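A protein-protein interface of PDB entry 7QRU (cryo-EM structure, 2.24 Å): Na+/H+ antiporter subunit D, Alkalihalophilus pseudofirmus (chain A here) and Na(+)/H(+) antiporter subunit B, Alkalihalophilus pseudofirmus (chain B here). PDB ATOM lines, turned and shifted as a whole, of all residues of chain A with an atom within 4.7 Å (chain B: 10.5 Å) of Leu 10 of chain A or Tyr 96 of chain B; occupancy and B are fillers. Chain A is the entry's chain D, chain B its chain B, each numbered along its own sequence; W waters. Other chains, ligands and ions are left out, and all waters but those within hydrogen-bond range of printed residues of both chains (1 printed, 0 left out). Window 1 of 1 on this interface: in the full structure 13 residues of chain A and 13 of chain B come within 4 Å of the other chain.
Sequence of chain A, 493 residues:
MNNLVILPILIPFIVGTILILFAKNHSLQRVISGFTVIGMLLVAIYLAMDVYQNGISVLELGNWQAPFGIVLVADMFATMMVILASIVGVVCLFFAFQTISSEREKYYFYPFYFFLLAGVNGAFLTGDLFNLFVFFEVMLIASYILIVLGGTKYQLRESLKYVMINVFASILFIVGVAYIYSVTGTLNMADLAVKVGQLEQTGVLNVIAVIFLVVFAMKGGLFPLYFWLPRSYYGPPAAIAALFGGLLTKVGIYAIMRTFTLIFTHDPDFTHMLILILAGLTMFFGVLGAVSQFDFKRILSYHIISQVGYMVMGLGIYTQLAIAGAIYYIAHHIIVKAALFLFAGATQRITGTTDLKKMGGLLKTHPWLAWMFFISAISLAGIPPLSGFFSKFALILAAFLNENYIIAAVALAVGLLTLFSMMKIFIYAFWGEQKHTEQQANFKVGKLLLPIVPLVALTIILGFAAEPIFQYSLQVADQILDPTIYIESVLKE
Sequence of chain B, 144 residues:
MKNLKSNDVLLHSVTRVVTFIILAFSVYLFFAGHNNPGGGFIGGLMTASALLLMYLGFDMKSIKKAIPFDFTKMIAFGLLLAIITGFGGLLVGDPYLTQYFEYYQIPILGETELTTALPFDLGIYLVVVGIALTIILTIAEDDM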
ATOM      1  N   ASN A   3       3.417  21.496   2.151  1.00  0.00           N
ATOM      2  CA  ASN A   3       3.109  20.873   3.413  1.00  0.00           C
ATOM      3  C   ASN A   3       1.888  21.506   4.105  1.00  0.00           C
ATOM      4  O   ASN A   3       1.233  20.875   4.937  1.00  0.00           O
ATOM      5  CB  ASN A   3       4.314  20.824   4.340  1.00  0.00           C
ATOM      6  CG  ASN A   3       5.242  19.640   4.165  1.00  0.00           C
ATOM      7  OD1 ASN A   3       4.783  18.521   4.031  1.00  0.00           O
ATOM      8  ND2 ASN A   3       6.544  19.837   4.247  1.00  0.00           N
ATOM      9  N   ILE A   6      -1.265  19.302   4.211  1.00  0.00           N
ATOM     10  CA  ILE A   6      -1.537  18.252   5.188  1.00  0.00           C
ATOM     11  C   ILE A   6      -1.986  18.803   6.539  1.00  0.00           C
ATOM     12  O   ILE A   6      -2.474  18.031   7.433  1.00  0.00           O
ATOM     13  CB  ILE A   6      -0.337  17.253   5.394  1.00  0.00           C
ATOM     14  CG1 ILE A   6      -0.881  15.930   5.970  1.00  0.00           C
ATOM     15  CG2 ILE A   6       0.724  17.869   6.300  1.00  0.00           C
ATOM     16  CD1 ILE A   6      -0.004  14.812   5.863  1.00  0.00           C
ATOM     17  N   LEU A   7      -1.936  20.121   6.731  1.00  0.00           N
ATOM     18  CA  LEU A   7      -2.272  20.648   8.048  1.00  0.00           C
ATOM     19  C   LEU A   7      -3.721  20.380   8.445  1.00  0.00           C
ATOM     20  O   LEU A   7      -3.980  20.106   9.627  1.00  0.00           O
ATOM     21  CB  LEU A   7      -1.954  22.120   8.117  1.00  0.00           C
ATOM     22  CG  LEU A   7      -0.491  22.509   8.194  1.00  0.00           C
ATOM     23  CD1 LEU A   7      -0.416  23.953   8.616  1.00  0.00           C
ATOM     24  CD2 LEU A   7       0.183  21.670   9.187  1.00  0.00           C
ATOM     25  N   PRO A   8      -4.729  20.483   7.559  1.00  0.00           N
ATOM     26  CA  PRO A   8      -6.080  20.108   7.961  1.00  0.00           C
ATOM     27  C   PRO A   8      -6.226  18.685   8.477  1.00  0.00           C
ATOM     28  O   PRO A   8      -7.044  18.446   9.281  1.00  0.00           O
ATOM     29  CB  PRO A   8      -6.868  20.247   6.658  1.00  0.00           C
ATOM     30  CG  PRO A   8      -6.101  21.240   5.854  1.00  0.00           C
ATOM     31  CD  PRO A   8      -4.660  20.993   6.205  1.00  0.00           C
ATOM     32  N   ILE A   9      -5.382  17.717   8.081  1.00  0.00           N
ATOM     33  CA  ILE A   9      -5.367  16.356   8.628  1.00  0.00           C
ATOM     34  C   ILE A   9      -4.551  16.329   9.904  1.00  0.00           C
ATOM     35  O   ILE A   9      -5.001  15.851  10.901  1.00  0.00           O
ATOM     36  CB  ILE A   9      -4.861  15.322   7.603  1.00  0.00           C
ATOM     37  CG1 ILE A   9      -5.598  15.550   6.260  1.00  0.00           C
ATOM     38  CG2 ILE A   9      -5.084  13.939   8.116  1.00  0.00           C
ATOM     39  CD1 ILE A   9      -4.943  15.022   5.056  1.00  0.00           C
ATOM     40  N   LEU A  10      -3.360  16.881   9.897  1.00  0.00           N
ATOM     41  CA  LEU A  10      -2.428  16.725  10.992  1.00  0.00           C
ATOM     42  C   LEU A  10      -2.796  17.523  12.242  1.00  0.00           C
ATOM     43  O   LEU A  10      -2.608  16.974  13.358  1.00  0.00           O
ATOM     44  CB  LEU A  10      -1.058  17.256  10.594  1.00  0.00           C
ATOM     45  CG  LEU A  10      -0.126  16.253   9.921  1.00  0.00           C
ATOM     46  CD1 LEU A  10       1.304  16.776   9.910  1.00  0.00           C
ATOM     47  CD2 LEU A  10      -0.180  14.909  10.618  1.00  0.00           C
ATOM     48  N   ILE A  11      -3.397  18.743  12.139  1.00  0.00           N
ATOM     49  CA  ILE A  11      -3.729  19.405  13.374  1.00  0.00           C
ATOM     50  C   ILE A  11      -4.700  18.554  14.191  1.00  0.00           C
ATOM     51  O   ILE A  11      -4.482  18.424  15.393  1.00  0.00           O
ATOM     52  CB  ILE A  11      -4.173  20.853  13.087  1.00  0.00           C
ATOM     53  CG1 ILE A  11      -2.959  21.655  12.632  1.00  0.00           C
ATOM     54  CG2 ILE A  11      -4.823  21.591  14.224  1.00  0.00           C
ATOM     55  CD1 ILE A  11      -3.435  22.984  11.943  1.00  0.00           C
ATOM     56  N   PRO A  12      -5.910  18.174  13.686  1.00  0.00           N
ATOM     57  CA  PRO A  12      -6.828  17.422  14.507  1.00  0.00           C
ATOM     58  C   PRO A  12      -6.198  16.092  14.933  1.00  0.00           C
ATOM     59  O   PRO A  12      -6.474  15.620  16.041  1.00  0.00           O
ATOM     60  CB  PRO A  12      -8.126  17.279  13.703  1.00  0.00           C
ATOM     61  CG  PRO A  12      -7.627  17.496  12.220  1.00  0.00           C
ATOM     62  CD  PRO A  12      -6.497  18.506  12.379  1.00  0.00           C
ATOM     63  N   PHE A  13      -5.448  15.440  14.056  1.00  0.00           N
ATOM     64  CA  PHE A  13      -4.791  14.202  14.464  1.00  0.00           C
ATOM     65  C   PHE A  13      -3.843  14.399  15.653  1.00  0.00           C
ATOM     66  O   PHE A  13      -3.945  13.659  16.659  1.00  0.00           O
ATOM     67  CB  PHE A  13      -4.131  13.599  13.242  1.00  0.00           C
ATOM     68  CG  PHE A  13      -3.530  12.241  13.412  1.00  0.00           C
ATOM     69  CD1 PHE A  13      -3.696  11.492  14.574  1.00  0.00           C
ATOM     70  CD2 PHE A  13      -2.836  11.689  12.353  1.00  0.00           C
ATOM     71  CE1 PHE A  13      -3.137  10.224  14.679  1.00  0.00           C
ATOM     72  CE2 PHE A  13      -2.322  10.396  12.456  1.00  0.00           C
ATOM     73  CZ  PHE A  13      -2.434   9.698  13.627  1.00  0.00           C
ATOM     74  N   ILE A  14      -2.978  15.424  15.599  1.00  0.00           N
ATOM     75  CA  ILE A  14      -2.070  15.687  16.720  1.00  0.00           C
ATOM     76  C   ILE A  14      -2.858  16.128  17.942  1.00  0.00           C
ATOM     77  O   ILE A  14      -2.591  15.639  19.064  1.00  0.00           O
ATOM     78  CB  ILE A  14      -1.006  16.734  16.380  1.00  0.00           C
ATOM     79  CG1 ILE A  14      -0.073  16.195  15.330  1.00  0.00           C
ATOM     80  CG2 ILE A  14      -0.224  17.120  17.582  1.00  0.00           C
ATOM     81  CD1 ILE A  14       0.779  17.255  14.693  1.00  0.00           C
ATOM     82  N   VAL A  15      -3.838  17.034  17.776  1.00  0.00           N
ATOM     83  CA  VAL A  15      -4.464  17.491  18.990  1.00  0.00           C
ATOM     84  C   VAL A  15      -5.338  16.379  19.602  1.00  0.00           C
ATOM     85  O   VAL A  15      -5.417  16.172  20.813  1.00  0.00           O
ATOM     86  CB  VAL A  15      -5.274  18.768  18.690  1.00  0.00           C
ATOM     87  CG1 VAL A  15      -6.232  19.067  19.812  1.00  0.00           C
ATOM     88  CG2 VAL A  15      -4.294  19.849  18.527  1.00  0.00           C
ATOM     89  N   LEU A  61       3.430  12.729  -0.356  1.00  0.00           N
ATOM     90  CA  LEU A  61       3.865  12.228   0.941  1.00  0.00           C
ATOM     91  C   LEU A  61       5.047  11.255   0.776  1.00  0.00           C
ATOM     92  O   LEU A  61       5.042  10.409  -0.112  1.00  0.00           O
ATOM     93  CB  LEU A  61       2.676  11.530   1.552  1.00  0.00           C
ATOM     94  CG  LEU A  61       1.560  12.485   1.978  1.00  0.00           C
ATOM     95  CD1 LEU A  61       0.474  11.713   2.584  1.00  0.00           C
ATOM     96  CD2 LEU A  61       2.043  13.446   3.005  1.00  0.00           C
ATOM     97  N   GLY A  62       6.128  11.492   1.529  1.00  0.00           N
ATOM     98  CA  GLY A  62       7.300  10.640   1.502  1.00  0.00           C
ATOM     99  C   GLY A  62       8.245  11.006   0.384  1.00  0.00           C
ATOM    100  O   GLY A  62       9.318  10.367   0.231  1.00  0.00           O
ATOM    101  N   GLY B  78       2.625   6.001  21.421  1.00  0.00           N
ATOM    102  CA  GLY B  78       2.736   5.392  20.107  1.00  0.00           C
ATOM    103  C   GLY B  78       2.330   6.278  18.958  1.00  0.00           C
ATOM    104  O   GLY B  78       3.124   6.470  18.034  1.00  0.00           O
ATOM    105  N   LEU B  79       1.119   6.854  19.046  1.00  0.00           N
ATOM    106  CA  LEU B  79       0.690   7.726  17.961  1.00  0.00           C
ATOM    107  C   LEU B  79       1.598   8.925  17.850  1.00  0.00           C
ATOM    108  O   LEU B  79       2.049   9.197  16.740  1.00  0.00           O
ATOM    109  CB  LEU B  79      -0.771   8.135  18.163  1.00  0.00           C
ATOM    110  CG  LEU B  79      -1.751   6.993  17.889  1.00  0.00           C
ATOM    111  CD1 LEU B  79      -3.116   7.302  18.420  1.00  0.00           C
ATOM    112  CD2 LEU B  79      -1.795   6.656  16.416  1.00  0.00           C
ATOM    113  N   LEU B  80       1.891   9.629  18.953  1.00  0.00           N
ATOM    114  CA  LEU B  80       2.779  10.785  18.791  1.00  0.00           C
ATOM    115  C   LEU B  80       4.153  10.406  18.283  1.00  0.00           C
ATOM    116  O   LEU B  80       4.648  11.068  17.427  1.00  0.00           O
ATOM    117  CB  LEU B  80       3.008  11.441  20.131  1.00  0.00           C
ATOM    118  CG  LEU B  80       1.775  12.147  20.653  1.00  0.00           C
ATOM    119  CD1 LEU B  80       2.049  12.591  22.062  1.00  0.00           C
ATOM    120  CD2 LEU B  80       1.406  13.249  19.737  1.00  0.00           C
ATOM    121  N   LEU B  81       4.739   9.290  18.703  1.00  0.00           N
ATOM    122  CA  LEU B  81       6.033   8.949  18.152  1.00  0.00           C
ATOM    123  C   LEU B  81       5.971   8.781  16.636  1.00  0.00           C
ATOM    124  O   LEU B  81       6.735   9.377  15.891  1.00  0.00           O
ATOM    125  CB  LEU B  81       6.537   7.697  18.828  1.00  0.00           C
ATOM    126  CG  LEU B  81       7.842   7.196  18.247  1.00  0.00           C
ATOM    127  CD1 LEU B  81       8.930   8.268  18.300  1.00  0.00           C
ATOM    128  CD2 LEU B  81       8.275   5.979  19.060  1.00  0.00           C
ATOM    129  N   ALA B  82       4.913   8.136  16.156  1.00  0.00           N
ATOM    130  CA  ALA B  82       4.781   7.954  14.726  1.00  0.00           C
ATOM    131  C   ALA B  82       4.497   9.257  14.002  1.00  0.00           C
ATOM    132  O   ALA B  82       5.101   9.508  12.960  1.00  0.00           O
ATOM    133  CB  ALA B  82       3.732   6.881  14.504  1.00  0.00           C
ATOM    134  N   ILE B  83       3.638  10.156  14.515  1.00  0.00           N
ATOM    135  CA  ILE B  83       3.466  11.473  13.865  1.00  0.00           C
ATOM    136  C   ILE B  83       4.752  12.315  13.843  1.00  0.00           C
ATOM    137  O   ILE B  83       5.188  12.884  12.836  1.00  0.00           O
ATOM    138  CB  ILE B  83       2.339  12.258  14.549  1.00  0.00           C
ATOM    139  CG1 ILE B  83       0.968  11.622  14.285  1.00  0.00           C
ATOM    140  CG2 ILE B  83       2.363  13.687  14.060  1.00  0.00           C
ATOM    141  CD1 ILE B  83      -0.023  11.824  15.374  1.00  0.00           C
ATOM    142  N   ILE B  84       5.419  12.378  14.954  1.00  0.00           N
ATOM    143  CA  ILE B  84       6.588  13.237  15.054  1.00  0.00           C
ATOM    144  C   ILE B  84       7.653  12.775  14.070  1.00  0.00           C
ATOM    145  O   ILE B  84       8.293  13.606  13.470  1.00  0.00           O
ATOM    146  CB  ILE B  84       7.104  13.271  16.516  1.00  0.00           C
ATOM    147  CG1 ILE B  84       6.105  13.899  17.485  1.00  0.00           C
ATOM    148  CG2 ILE B  84       8.385  13.990  16.644  1.00  0.00           C
ATOM    149  CD1 ILE B  84       5.558  15.220  17.006  1.00  0.00           C
ATOM    150  N   THR B  85       7.948  11.478  13.998  1.00  0.00           N
ATOM    151  CA  THR B  85       8.924  10.938  13.065  1.00  0.00           C
ATOM    152  C   THR B  85       8.690  11.472  11.640  1.00  0.00           C
ATOM    153  O   THR B  85       9.624  11.793  10.904  1.00  0.00           O
ATOM    154  CB  THR B  85       8.904   9.402  13.097  1.00  0.00           C
ATOM    155  OG1 THR B  85       9.336   8.982  14.375  1.00  0.00           O
ATOM    156  CG2 THR B  85       9.787   8.789  12.044  1.00  0.00           C
ATOM    157  N   GLY B  86       7.420  11.583  11.248  1.00  0.00           N
ATOM    158  CA  GLY B  86       7.036  12.136   9.965  1.00  0.00           C
ATOM    159  C   GLY B  86       7.449  13.581   9.710  1.00  0.00           C
ATOM    160  O   GLY B  86       7.460  13.980   8.571  1.00  0.00           O
ATOM    161  N   PHE B  87       7.834  14.365  10.722  1.00  0.00           N
ATOM    162  CA  PHE B  87       8.238  15.766  10.495  1.00  0.00           C
ATOM    163  C   PHE B  87       9.720  15.909  10.190  1.00  0.00           C
ATOM    164  O   PHE B  87      10.138  16.993   9.808  1.00  0.00           O
ATOM    165  CB  PHE B  87       7.980  16.628  11.721  1.00  0.00           C
ATOM    166  CG  PHE B  87       6.521  16.907  11.943  1.00  0.00           C
ATOM    167  CD1 PHE B  87       5.853  17.773  11.106  1.00  0.00           C
ATOM    168  CD2 PHE B  87       5.842  16.342  12.988  1.00  0.00           C
ATOM    169  CE1 PHE B  87       4.517  18.035  11.314  1.00  0.00           C
ATOM    170  CE2 PHE B  87       4.505  16.623  13.192  1.00  0.00           C
ATOM    171  CZ  PHE B  87       3.861  17.460  12.369  1.00  0.00           C
ATOM    172  N   GLY B  88      10.505  14.824  10.352  1.00  0.00           N
ATOM    173  CA  GLY B  88      11.872  14.734   9.878  1.00  0.00           C
ATOM    174  C   GLY B  88      12.161  15.538   8.627  1.00  0.00           C
ATOM    175  O   GLY B  88      13.085  16.313   8.586  1.00  0.00           O
ATOM    176  N   GLY B  89      11.376  15.341   7.593  1.00  0.00           N
ATOM    177  CA  GLY B  89      11.651  16.025   6.354  1.00  0.00           C
ATOM    178  C   GLY B  89      11.455  17.526   6.478  1.00  0.00           C
ATOM    179  O   GLY B  89      12.015  18.257   5.671  1.00  0.00           O
ATOM    180  N   LEU B  90      10.621  18.015   7.402  1.00  0.00           N
ATOM    181  CA  LEU B  90      10.463  19.473   7.502  1.00  0.00           C
ATOM    182  C   LEU B  90      11.763  20.161   7.946  1.00  0.00           C
ATOM    183  O   LEU B  90      11.931  21.339   7.643  1.00  0.00           O
ATOM    184  CB  LEU B  90       9.271  19.869   8.382  1.00  0.00           C
ATOM    185  CG  LEU B  90       7.944  19.685   7.639  1.00  0.00           C
ATOM    186  CD1 LEU B  90       7.571  18.223   7.428  1.00  0.00           C
ATOM    187  CD2 LEU B  90       6.807  20.332   8.370  1.00  0.00           C
ATOM    188  N   LEU B  91      12.715  19.436   8.549  1.00  0.00           N
ATOM    189  CA  LEU B  91      14.090  19.912   8.738  1.00  0.00           C
ATOM    190  C   LEU B  91      14.822  20.175   7.436  1.00  0.00           C
ATOM    191  O   LEU B  91      15.637  21.106   7.365  1.00  0.00           O
ATOM    192  CB  LEU B  91      14.955  18.907   9.503  1.00  0.00           C
ATOM    193  CG  LEU B  91      14.898  19.022  11.028  1.00  0.00           C
ATOM    194  CD1 LEU B  91      13.477  19.243  11.536  1.00  0.00           C
ATOM    195  CD2 LEU B  91      15.488  17.770  11.666  1.00  0.00           C
ATOM    196  N   VAL B  92      14.640  19.318   6.440  1.00  0.00           N
ATOM    197  CA  VAL B  92      15.481  19.423   5.254  1.00  0.00           C
ATOM    198  C   VAL B  92      14.632  19.908   4.078  1.00  0.00           C
ATOM    199  O   VAL B  92      14.999  19.726   2.926  1.00  0.00           O
ATOM    200  CB  VAL B  92      16.209  18.094   5.008  1.00  0.00           C
ATOM    201  CG1 VAL B  92      15.222  16.958   4.805  1.00  0.00           C
ATOM    202  CG2 VAL B  92      17.186  18.179   3.839  1.00  0.00           C
ATOM    203  N   GLY B  93      13.477  20.520   4.402  1.00  0.00           N
ATOM    204  CA  GLY B  93      12.544  21.046   3.420  1.00  0.00           C
ATOM    205  C   GLY B  93      11.969  19.976   2.492  1.00  0.00           C
ATOM    206  O   GLY B  93      12.155  20.049   1.287  1.00  0.00           O
ATOM    207  N   ASP B  94      11.332  18.964   3.087  1.00  0.00           N
ATOM    208  CA  ASP B  94      10.864  17.799   2.368  1.00  0.00           C
ATOM    209  C   ASP B  94       9.421  17.521   2.769  1.00  0.00           C
ATOM    210  O   ASP B  94       8.919  17.854   3.820  1.00  0.00           O
ATOM    211  CB  ASP B  94      11.691  16.560   2.637  1.00  0.00           C
ATOM    212  CG  ASP B  94      12.771  16.343   1.612  1.00  0.00           C
ATOM    213  OD1 ASP B  94      12.798  17.137   0.646  1.00  0.00           O
ATOM    214  OD2 ASP B  94      13.609  15.378   1.798  1.00  0.00           O
ATOM    215  N   PRO B  95       8.667  16.848   1.932  1.00  0.00           N
ATOM    216  CA  PRO B  95       7.300  16.630   2.326  1.00  0.00           C
ATOM    217  C   PRO B  95       7.156  15.820   3.599  1.00  0.00           C
ATOM    218  O   PRO B  95       8.058  15.111   3.948  1.00  0.00           O
ATOM    219  CB  PRO B  95       6.729  15.872   1.170  1.00  0.00           C
ATOM    220  CG  PRO B  95       7.783  15.807   0.151  1.00  0.00           C
ATOM    221  CD  PRO B  95       9.108  16.323   0.653  1.00  0.00           C
ATOM    222  N   TYR B  96       6.060  15.990   4.325  1.00  0.00           N
ATOM    223  CA  TYR B  96       5.775  15.179   5.516  1.00  0.00           C
ATOM    224  C   TYR B  96       5.908  13.685   5.179  1.00  0.00           C
ATOM    225  O   TYR B  96       5.573  13.252   4.060  1.00  0.00           O
ATOM    226  CB  TYR B  96       4.367  15.451   6.021  1.00  0.00           C
ATOM    227  CG  TYR B  96       4.013  14.708   7.265  1.00  0.00           C
ATOM    228  CD1 TYR B  96       4.453  15.173   8.528  1.00  0.00           C
ATOM    229  CD2 TYR B  96       3.145  13.622   7.217  1.00  0.00           C
ATOM    230  CE1 TYR B  96       4.140  14.553   9.714  1.00  0.00           C
ATOM    231  CE2 TYR B  96       2.816  12.968   8.424  1.00  0.00           C
ATOM    232  CZ  TYR B  96       3.380  13.391   9.637  1.00  0.00           C
ATOM    233  OH  TYR B  96       3.094  12.783  10.833  1.00  0.00           O
ATOM    234  N   LEU B  97       6.438  12.926   6.118  1.00  0.00           N
ATOM    235  CA  LEU B  97       6.565  11.498   6.082  1.00  0.00           C
ATOM    236  C   LEU B  97       7.644  11.074   5.096  1.00  0.00           C
ATOM    237  O   LEU B  97       7.583   9.967   4.618  1.00  0.00           O
ATOM    238  CB  LEU B  97       5.184  10.897   5.792  1.00  0.00           C
ATOM    239  CG  LEU B  97       4.609  10.178   7.026  1.00  0.00           C
ATOM    240  CD1 LEU B  97       3.235   9.615   6.765  1.00  0.00           C
ATOM    241  CD2 LEU B  97       5.510   9.059   7.421  1.00  0.00           C
ATOM    242  N   THR B  98       8.587  11.949   4.733  1.00  0.00           N
ATOM    243  CA  THR B  98       9.802  11.501   4.080  1.00  0.00           C
ATOM    244  C   THR B  98      10.683  10.715   5.046  1.00  0.00           C
ATOM    245  O   THR B  98      10.613  10.994   6.226  1.00  0.00           O
ATOM    246  CB  THR B  98      10.491  12.681   3.456  1.00  0.00           C
ATOM    247  OG1 THR B  98       9.660  13.437   2.582  1.00  0.00           O
ATOM    248  CG2 THR B  98      11.585  12.192   2.578  1.00  0.00           C
ATOM    249  N   GLN B  99      11.210   9.563   4.634  1.00  0.00           N
ATOM    250  CA  GLN B  99      11.957   8.622   5.490  1.00  0.00           C
ATOM    251  C   GLN B  99      13.385   8.724   4.989  1.00  0.00           C
ATOM    252  O   GLN B  99      13.602   9.111   3.850  1.00  0.00           O
ATOM    253  CB  GLN B  99      11.447   7.180   5.376  1.00  0.00           C
ATOM    254  CG  GLN B  99      10.028   6.875   5.840  1.00  0.00           C
ATOM    255  CD  GLN B  99       9.691   7.046   7.310  1.00  0.00           C
ATOM    256  OE1 GLN B  99      10.385   7.724   8.062  1.00  0.00           O
ATOM    257  NE2 GLN B  99       8.601   6.417   7.765  1.00  0.00           N
ATOM    258  N   TYR B 100      14.341   8.542   5.870  1.00  0.00           N
ATOM    259  CA  TYR B 100      15.771   8.714   5.602  1.00  0.00           C
ATOM    260  C   TYR B 100      16.555   7.519   6.126  1.00  0.00           C
ATOM    261  O   TYR B 100      16.144   6.963   7.152  1.00  0.00           O
ATOM    262  CB  TYR B 100      16.224   9.947   6.368  1.00  0.00           C
ATOM    263  CG  TYR B 100      15.546  11.183   5.854  1.00  0.00           C
ATOM    264  CD1 TYR B 100      15.892  11.673   4.603  1.00  0.00           C
ATOM    265  CD2 TYR B 100      14.481  11.780   6.545  1.00  0.00           C
ATOM    266  CE1 TYR B 100      15.292  12.819   4.082  1.00  0.00           C
ATOM    267  CE2 TYR B 100      13.808  12.857   5.980  1.00  0.00           C
ATOM    268  CZ  TYR B 100      14.242  13.406   4.761  1.00  0.00           C
ATOM    269  OH  TYR B 100      13.582  14.461   4.151  1.00  0.00           O
ATOM    270  N   THR B 116      14.807   6.499   9.712  1.00  0.00           N
ATOM    271  CA  THR B 116      13.649   7.049  10.460  1.00  0.00           C
ATOM    272  C   THR B 116      12.515   6.035  10.526  1.00  0.00           C
ATOM    273  O   THR B 116      11.729   6.040  11.445  1.00  0.00           O
ATOM    274  CB  THR B 116      13.177   8.303   9.741  1.00  0.00           C
ATOM    275  OG1 THR B 116      12.997   8.030   8.319  1.00  0.00           O
ATOM    276  CG2 THR B 116      14.291   9.310   9.863  1.00  0.00           C
ATOM    277  N   PHE B 120       9.561   5.194  13.337  1.00  0.00           N
ATOM    278  CA  PHE B 120       8.197   5.247  12.868  1.00  0.00           C
ATOM    279  C   PHE B 120       7.515   3.938  13.203  1.00  0.00           C
ATOM    280  O   PHE B 120       6.387   3.914  13.703  1.00  0.00           O
ATOM    281  CB  PHE B 120       8.181   5.478  11.357  1.00  0.00           C
ATOM    282  CG  PHE B 120       6.805   5.444  10.782  1.00  0.00           C
ATOM    283  CD1 PHE B 120       5.970   6.529  10.910  1.00  0.00           C
ATOM    284  CD2 PHE B 120       6.305   4.294  10.189  1.00  0.00           C
ATOM    285  CE1 PHE B 120       4.692   6.515  10.351  1.00  0.00           C
ATOM    286  CE2 PHE B 120       5.047   4.311   9.593  1.00  0.00           C
ATOM    287  CZ  PHE B 120       4.249   5.437   9.663  1.00  0.00           C
ATOM    288  N   ILE B 124       4.230   2.493  15.598  1.00  0.00           N
ATOM    289  CA  ILE B 124       3.191   1.542  15.221  1.00  0.00           C
ATOM    290  C   ILE B 124       3.128   0.410  16.259  1.00  0.00           C
ATOM    291  O   ILE B 124       2.067   0.041  16.685  1.00  0.00           O
ATOM    292  CB  ILE B 124       3.439   0.927  13.837  1.00  0.00           C
ATOM    293  CG1 ILE B 124       3.569   1.958  12.722  1.00  0.00           C
ATOM    294  CG2 ILE B 124       2.438  -0.221  13.527  1.00  0.00           C
ATOM    295  CD1 ILE B 124       2.665   3.190  12.866  1.00  0.00           C
HETATM  296  O   HOH W   1      10.296   8.540   2.302  1.00  0.00           O
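The backbone carbonyl oxygen (O) of Asp 94 of chain B lies within hydrogen-bond range of the side-chain amide nitrogen (ND2) of Asn 3 of chain A (3.1 Å).
The side-chain amide oxygen of Asn 3 of chain A is in hydrogen-bond range of the backbone NH of Tyr 96 of chain B.
The backbone NH (N) of Gly 62 of chain A sits at hydrogen-bond distance from the backbone carbonyl oxygen (O) of Tyr 96 of chain B.
O of Ile 83 of chain B is in hydrogen-bond range of OH of Tyr 96 of chain B (2.9 Å).
The backbone carbonyl oxygen of Gly 86 of chain B sits at hydrogen-bond distance from the backbone NH of Leu 97 of chain B.
O of Gly 89 of chain B lies within hydrogen-bond range of N of Asp 94 of chain B, 2.8 Å away.
O of Pro 95 of chain B sits at hydrogen-bond distance from OG1 of Thr 98 of chain B, 2.7 Å away.
Among the printed residues, merely in contact across the chains: Gly 62 of chain A with Leu 97 of chain B, Phe 13 of chain A with Ile 83 of chain B, Gly 62 of chain A with Thr 98 of chain B, Asn 3 of chain A with Pro 95 of chain B, Leu 10 of chain A with Tyr 96 of chain B, Leu 10 of chain A with Phe 87 of chain B, Ile 6 of chain A with Tyr 96 of chain B, Asn 3 of chain A with Leu 90 of chain B, Leu 61 of chain A with Tyr 96 of chain B, Ile 14 of chain A with Ile 83 of chain B and Ile 14 of chain A with Phe 87 of chain B.
No residue of chain B comes within 4 Å of Ile 9 of chain A.
Leu 10 of chain A touches just these residues of chain B: Phe 87 (3.6 Å) and Tyr 96 (3.6 Å).
No residue of chain B comes within 4 Å of Ile 11 of chain A.
Pro 12 of chain A touches none of the printed residues of chain B.
Printed residues of chain B within 4 Å of Gly 62 of chain A: Tyr 96, Leu 97 and Thr 98.
Leu 81 of chain B touches none of the printed residues of chain A.
Ala 82 of chain B touches none of the printed residues of chain A.
Printed residues of chain A within 4 Å of Leu 90 of chain B: Asn 3.
Printed residues of chain A within 4 Å of Asp 94 of chain B: Asn 3.
Of the printed residues of chain A, Pro 95 of chain B touches Asn 3 (3.6 Å).
Tyr 96 of chain B touches just these residues of chain A: Asn 3, Ile 6, Leu 10, Leu 61 and Gly 62.
The nearest residue of chain B that does not touch Leu 10 of chain A is Ile 83 of chain B (4.5 Å).
The nearest printed residue of chain A that does not touch Tyr 96 of chain B is Phe 13 of chain A (6.1 Å).
Hydrophobic or aromatic side chains of chain A within 4 Å of the printed part of chain B: Ile 6, Leu 10, Phe 13, Ile 14 and Leu 61.
Of the 26 printed residues of chain B, 8 touch a printed residue of chain A.
Water W1 bridges N of Gln 99 of chain B (2.7 Å) and O of Gly 62 of chain A (2.9 Å).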
